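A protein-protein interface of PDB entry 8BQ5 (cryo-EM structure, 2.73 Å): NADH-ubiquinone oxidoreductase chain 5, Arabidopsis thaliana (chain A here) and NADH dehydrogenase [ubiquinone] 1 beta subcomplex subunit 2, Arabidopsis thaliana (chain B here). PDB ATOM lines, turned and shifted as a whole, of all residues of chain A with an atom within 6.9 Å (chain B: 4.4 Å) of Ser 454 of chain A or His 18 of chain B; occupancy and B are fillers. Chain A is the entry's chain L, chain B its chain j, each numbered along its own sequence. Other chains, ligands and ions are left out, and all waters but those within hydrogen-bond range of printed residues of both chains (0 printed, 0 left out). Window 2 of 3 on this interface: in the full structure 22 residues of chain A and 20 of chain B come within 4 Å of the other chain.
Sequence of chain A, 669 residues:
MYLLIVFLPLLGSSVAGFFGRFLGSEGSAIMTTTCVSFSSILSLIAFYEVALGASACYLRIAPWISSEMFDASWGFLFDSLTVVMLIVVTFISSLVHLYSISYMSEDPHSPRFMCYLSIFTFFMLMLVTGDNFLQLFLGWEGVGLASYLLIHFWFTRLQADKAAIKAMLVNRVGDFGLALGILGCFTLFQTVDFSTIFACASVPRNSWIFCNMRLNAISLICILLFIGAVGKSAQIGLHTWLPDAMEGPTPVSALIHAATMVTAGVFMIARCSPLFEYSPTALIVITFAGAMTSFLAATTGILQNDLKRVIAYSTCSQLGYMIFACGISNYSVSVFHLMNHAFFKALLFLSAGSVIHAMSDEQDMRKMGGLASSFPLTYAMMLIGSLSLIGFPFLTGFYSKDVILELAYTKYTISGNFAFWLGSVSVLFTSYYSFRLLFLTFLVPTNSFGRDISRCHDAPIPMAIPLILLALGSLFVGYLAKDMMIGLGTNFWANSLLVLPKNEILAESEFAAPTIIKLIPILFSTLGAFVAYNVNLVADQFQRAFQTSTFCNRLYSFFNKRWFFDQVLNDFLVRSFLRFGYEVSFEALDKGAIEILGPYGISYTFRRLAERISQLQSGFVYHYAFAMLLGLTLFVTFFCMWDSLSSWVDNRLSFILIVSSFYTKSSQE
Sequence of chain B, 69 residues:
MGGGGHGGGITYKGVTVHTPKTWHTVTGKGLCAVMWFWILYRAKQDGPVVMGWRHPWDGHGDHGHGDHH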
ATOM      1  N   SER A 373     -10.505   6.753  24.374  1.00  0.00           N
ATOM      2  CA  SER A 373      -9.599   6.552  23.219  1.00  0.00           C
ATOM      3  C   SER A 373      -9.857   5.185  22.588  1.00  0.00           C
ATOM      4  O   SER A 373      -9.730   5.080  21.359  1.00  0.00           O
ATOM      5  CB  SER A 373      -8.175   6.649  23.664  1.00  0.00           C
ATOM      6  OG  SER A 373      -7.990   7.750  24.540  1.00  0.00           O
ATOM      7  N   SER A 374     -10.213   4.185  23.399  1.00  0.00           N
ATOM      8  CA  SER A 374     -10.387   2.803  22.883  1.00  0.00           C
ATOM      9  C   SER A 374     -11.595   2.719  21.944  1.00  0.00           C
ATOM     10  O   SER A 374     -11.577   1.855  21.055  1.00  0.00           O
ATOM     11  CB  SER A 374     -10.497   1.823  24.016  1.00  0.00           C
ATOM     12  OG  SER A 374      -9.445   2.009  24.951  1.00  0.00           O
ATOM     13  N   PHE A 449     -12.135  -4.421  34.197  1.00  0.00           N
ATOM     14  CA  PHE A 449     -11.340  -5.624  34.392  1.00  0.00           C
ATOM     15  C   PHE A 449     -10.327  -5.788  33.268  1.00  0.00           C
ATOM     16  O   PHE A 449     -10.553  -5.336  32.142  1.00  0.00           O
ATOM     17  CB  PHE A 449     -12.239  -6.858  34.456  1.00  0.00           C
ATOM     18  CG  PHE A 449     -13.009  -6.985  35.735  1.00  0.00           C
ATOM     19  CD1 PHE A 449     -12.430  -7.566  36.849  1.00  0.00           C
ATOM     20  CD2 PHE A 449     -14.312  -6.530  35.824  1.00  0.00           C
ATOM     21  CE1 PHE A 449     -13.137  -7.691  38.025  1.00  0.00           C
ATOM     22  CE2 PHE A 449     -15.025  -6.652  36.999  1.00  0.00           C
ATOM     23  CZ  PHE A 449     -14.436  -7.233  38.101  1.00  0.00           C
ATOM     24  N   GLY A 450      -9.216  -6.457  33.580  1.00  0.00           N
ATOM     25  CA  GLY A 450      -8.165  -6.632  32.592  1.00  0.00           C
ATOM     26  C   GLY A 450      -8.607  -7.432  31.383  1.00  0.00           C
ATOM     27  O   GLY A 450      -8.292  -7.081  30.244  1.00  0.00           O
ATOM     28  N   ARG A 451      -9.343  -8.522  31.611  1.00  0.00           N
ATOM     29  CA  ARG A 451      -9.781  -9.352  30.492  1.00  0.00           C
ATOM     30  C   ARG A 451     -10.825  -8.639  29.643  1.00  0.00           C
ATOM     31  O   ARG A 451     -11.018  -8.990  28.473  1.00  0.00           O
ATOM     32  CB  ARG A 451     -10.323 -10.684  31.008  1.00  0.00           C
ATOM     33  CG  ARG A 451     -10.787 -11.641  29.922  1.00  0.00           C
ATOM     34  CD  ARG A 451     -11.294 -12.961  30.502  1.00  0.00           C
ATOM     35  NE  ARG A 451     -11.753 -13.916  29.500  1.00  0.00           N
ATOM     36  CZ  ARG A 451     -12.978 -13.946  28.992  1.00  0.00           C
ATOM     37  NH1 ARG A 451     -13.903 -13.076  29.365  1.00  0.00           N
ATOM     38  NH2 ARG A 451     -13.279 -14.870  28.086  1.00  0.00           N
ATOM     39  N   ASP A 452     -11.500  -7.639  30.209  1.00  0.00           N
ATOM     40  CA  ASP A 452     -12.493  -6.894  29.443  1.00  0.00           C
ATOM     41  C   ASP A 452     -11.835  -5.982  28.414  1.00  0.00           C
ATOM     42  O   ASP A 452     -12.266  -5.936  27.255  1.00  0.00           O
ATOM     43  CB  ASP A 452     -13.381  -6.090  30.391  1.00  0.00           C
ATOM     44  CG  ASP A 452     -14.383  -6.958  31.130  1.00  0.00           C
ATOM     45  OD1 ASP A 452     -14.292  -8.198  31.021  1.00  0.00           O
ATOM     46  OD2 ASP A 452     -15.260  -6.399  31.821  1.00  0.00           O
ATOM     47  N   ILE A 453     -10.784  -5.271  28.827  1.00  0.00           N
ATOM     48  CA  ILE A 453     -10.127  -4.290  27.906  1.00  0.00           C
ATOM     49  C   ILE A 453      -9.302  -5.044  26.854  1.00  0.00           C
ATOM     50  O   ILE A 453      -9.042  -4.459  25.781  1.00  0.00           O
ATOM     51  CB  ILE A 453      -9.297  -3.257  28.699  1.00  0.00           C
ATOM     52  CG1 ILE A 453     -10.130  -2.598  29.798  1.00  0.00           C
ATOM     53  CG2 ILE A 453      -8.691  -2.209  27.781  1.00  0.00           C
ATOM     54  CD1 ILE A 453     -11.304  -1.819  29.265  1.00  0.00           C
ATOM     55  N   SER A 454      -8.920  -6.291  27.130  1.00  0.00           N
ATOM     56  CA  SER A 454      -8.160  -7.100  26.186  1.00  0.00           C
ATOM     57  C   SER A 454      -9.010  -7.652  25.049  1.00  0.00           C
ATOM     58  O   SER A 454      -8.450  -8.207  24.097  1.00  0.00           O
ATOM     59  CB  SER A 454      -7.473  -8.255  26.918  1.00  0.00           C
ATOM     60  OG  SER A 454      -6.501  -7.775  27.830  1.00  0.00           O
ATOM     61  N   ARG A 455     -10.337  -7.526  25.122  1.00  0.00           N
ATOM     62  CA  ARG A 455     -11.221  -8.092  24.110  1.00  0.00           C
ATOM     63  C   ARG A 455     -12.186  -7.054  23.547  1.00  0.00           C
ATOM     64  O   ARG A 455     -13.284  -7.413  23.108  1.00  0.00           O
ATOM     65  CB  ARG A 455     -11.998  -9.281  24.683  1.00  0.00           C
ATOM     66  CG  ARG A 455     -11.111 -10.384  25.232  1.00  0.00           C
ATOM     67  CD  ARG A 455     -11.912 -11.443  25.973  1.00  0.00           C
ATOM     68  NE  ARG A 455     -12.067 -12.661  25.186  1.00  0.00           N
ATOM     69  CZ  ARG A 455     -11.543 -13.834  25.514  1.00  0.00           C
ATOM     70  NH1 ARG A 455     -10.809 -13.980  26.606  1.00  0.00           N
ATOM     71  NH2 ARG A 455     -11.753 -14.883  24.725  1.00  0.00           N
ATOM     72  N   CYS A 456     -11.807  -5.781  23.553  1.00  0.00           N
ATOM     73  CA  CYS A 456     -12.676  -4.736  23.037  1.00  0.00           C
ATOM     74  C   CYS A 456     -12.599  -4.661  21.515  1.00  0.00           C
ATOM     75  O   CYS A 456     -11.570  -4.954  20.899  1.00  0.00           O
ATOM     76  CB  CYS A 456     -12.307  -3.378  23.632  1.00  0.00           C
ATOM     77  SG  CYS A 456     -12.427  -3.271  25.426  1.00  0.00           S
ATOM     78  N   GLY B   9      -1.794  -3.811  18.381  1.00  0.00           N
ATOM     79  CA  GLY B   9      -2.077  -3.519  19.775  1.00  0.00           C
ATOM     80  C   GLY B   9      -0.830  -3.330  20.618  1.00  0.00           C
ATOM     81  O   GLY B   9       0.239  -3.836  20.279  1.00  0.00           O
ATOM     82  N   VAL B  15      -2.089  -6.765  29.975  1.00  0.00           N
ATOM     83  CA  VAL B  15      -3.258  -6.177  29.333  1.00  0.00           C
ATOM     84  C   VAL B  15      -2.866  -5.657  27.957  1.00  0.00           C
ATOM     85  O   VAL B  15      -1.811  -5.033  27.783  1.00  0.00           O
ATOM     86  CB  VAL B  15      -3.880  -5.081  30.217  1.00  0.00           C
ATOM     87  CG1 VAL B  15      -3.932  -5.557  31.658  1.00  0.00           C
ATOM     88  CG2 VAL B  15      -3.107  -3.776  30.127  1.00  0.00           C
ATOM     89  N   THR B  16      -3.686  -5.971  26.963  1.00  0.00           N
ATOM     90  CA  THR B  16      -3.483  -5.536  25.592  1.00  0.00           C
ATOM     91  C   THR B  16      -4.700  -4.739  25.153  1.00  0.00           C
ATOM     92  O   THR B  16      -5.835  -5.197  25.315  1.00  0.00           O
ATOM     93  CB  THR B  16      -3.269  -6.732  24.660  1.00  0.00           C
ATOM     94  OG1 THR B  16      -2.118  -7.475  25.082  1.00  0.00           O
ATOM     95  CG2 THR B  16      -3.066  -6.266  23.229  1.00  0.00           C
ATOM     96  N   VAL B  17      -4.469  -3.546  24.617  1.00  0.00           N
ATOM     97  CA  VAL B  17      -5.529  -2.711  24.066  1.00  0.00           C
ATOM     98  C   VAL B  17      -5.228  -2.475  22.594  1.00  0.00           C
ATOM     99  O   VAL B  17      -4.232  -1.826  22.250  1.00  0.00           O
ATOM    100  CB  VAL B  17      -5.671  -1.387  24.839  1.00  0.00           C
ATOM    101  CG1 VAL B  17      -4.310  -0.795  25.151  1.00  0.00           C
ATOM    102  CG2 VAL B  17      -6.528  -0.399  24.058  1.00  0.00           C
ATOM    103  N   HIS B  18      -6.075  -3.019  21.727  1.00  0.00           N
ATOM    104  CA  HIS B  18      -5.873  -2.922  20.291  1.00  0.00           C
ATOM    105  C   HIS B  18      -6.172  -1.508  19.810  1.00  0.00           C
ATOM    106  O   HIS B  18      -7.094  -0.851  20.299  1.00  0.00           O
ATOM    107  CB  HIS B  18      -6.751  -3.928  19.542  1.00  0.00           C
ATOM    108  CG  HIS B  18      -6.513  -5.356  19.931  1.00  0.00           C
ATOM    109  ND1 HIS B  18      -6.505  -5.786  21.241  1.00  0.00           N
ATOM    110  CD2 HIS B  18      -6.275  -6.455  19.176  1.00  0.00           C
ATOM    111  CE1 HIS B  18      -6.274  -7.087  21.275  1.00  0.00           C
ATOM    112  NE2 HIS B  18      -6.131  -7.517  20.036  1.00  0.00           N
ATOM    113  N   THR B  19      -5.375  -1.046  18.853  1.00  0.00           N
ATOM    114  CA  THR B  19      -5.590   0.268  18.271  1.00  0.00           C
ATOM    115  C   THR B  19      -6.908   0.282  17.499  1.00  0.00           C
ATOM    116  O   THR B  19      -7.182  -0.640  16.724  1.00  0.00           O
ATOM    117  CB  THR B  19      -4.433   0.632  17.338  1.00  0.00           C
ATOM    118  OG1 THR B  19      -3.211   0.094  17.857  1.00  0.00           O
ATOM    119  CG2 THR B  19      -4.294   2.142  17.208  1.00  0.00           C
ATOM    120  N   PRO B  20      -7.746   1.296  17.693  1.00  0.00           N
ATOM    121  CA  PRO B  20      -8.987   1.380  16.920  1.00  0.00           C
ATOM    122  C   PRO B  20      -8.704   1.585  15.441  1.00  0.00           C
ATOM    123  O   PRO B  20      -7.686   2.156  15.046  1.00  0.00           O
ATOM    124  CB  PRO B  20      -9.704   2.591  17.524  1.00  0.00           C
ATOM    125  CG  PRO B  20      -8.609   3.432  18.068  1.00  0.00           C
ATOM    126  CD  PRO B  20      -7.547   2.481  18.546  1.00  0.00           C
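The side-chain hydroxyl (OG) of Ser 454 of chain A lies within hydrogen-bond range of the backbone NH (N) of Thr 16 of chain B. The backbone carbonyl oxygen of Thr 16 of chain B lies close to the backbone carbonyl oxygen of Ile 453 of chain A.
Of the 7 printed residues of chain B, 5 touch a printed residue of chain A. Printed residues of chain B that touch a printed residue of chain A: Val 15, Thr 16, Val 17, His 18 and Pro 20. Among the printed residues, no Asp or Glu carboxylate lies within 4 Å of a Lys or Arg side-chain nitrogen of the other chain.
O of Ile 453 of chain A sits close to SG of Cys 456 of chain A (3.6 Å). The backbone carbonyl oxygen (O) of Gly 450 of chain A is in hydrogen-bond range of the side-chain hydroxyl (OG) of Ser 454 of chain A, at 3.1 Å.
Ser 454 of chain A touches just these residues of chain B: Val 15, Thr 16 and His 18. His 18 of chain B touches one residue of chain A. Of the printed residues of chain B, Ser 374 of chain A touches Val 17. Of the printed residues of chain A, Pro 20 of chain B touches Ser 373. Phe 449 of chain A touches none of the printed residues of chain B. The nearest printed residue of chain B that does not touch Ser 454 of chain A is Val 17 of chain B (5.4 Å). The nearest printed residue of chain B that does not touch Ile 453 of chain A is Val 17 of chain B (4.3 Å).
Among the printed residues, pairs that only touch across the chains: Ser 454 of chain A with His 18 of chain B (3.7 Å), Ser 373 of chain A with Pro 20 of chain B (3.8 Å), Ser 374 of chain A with Val 17 of chain B (3.9 Å) and Ser 454 of chain A with Val 15 of chain B (3.9 Å).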
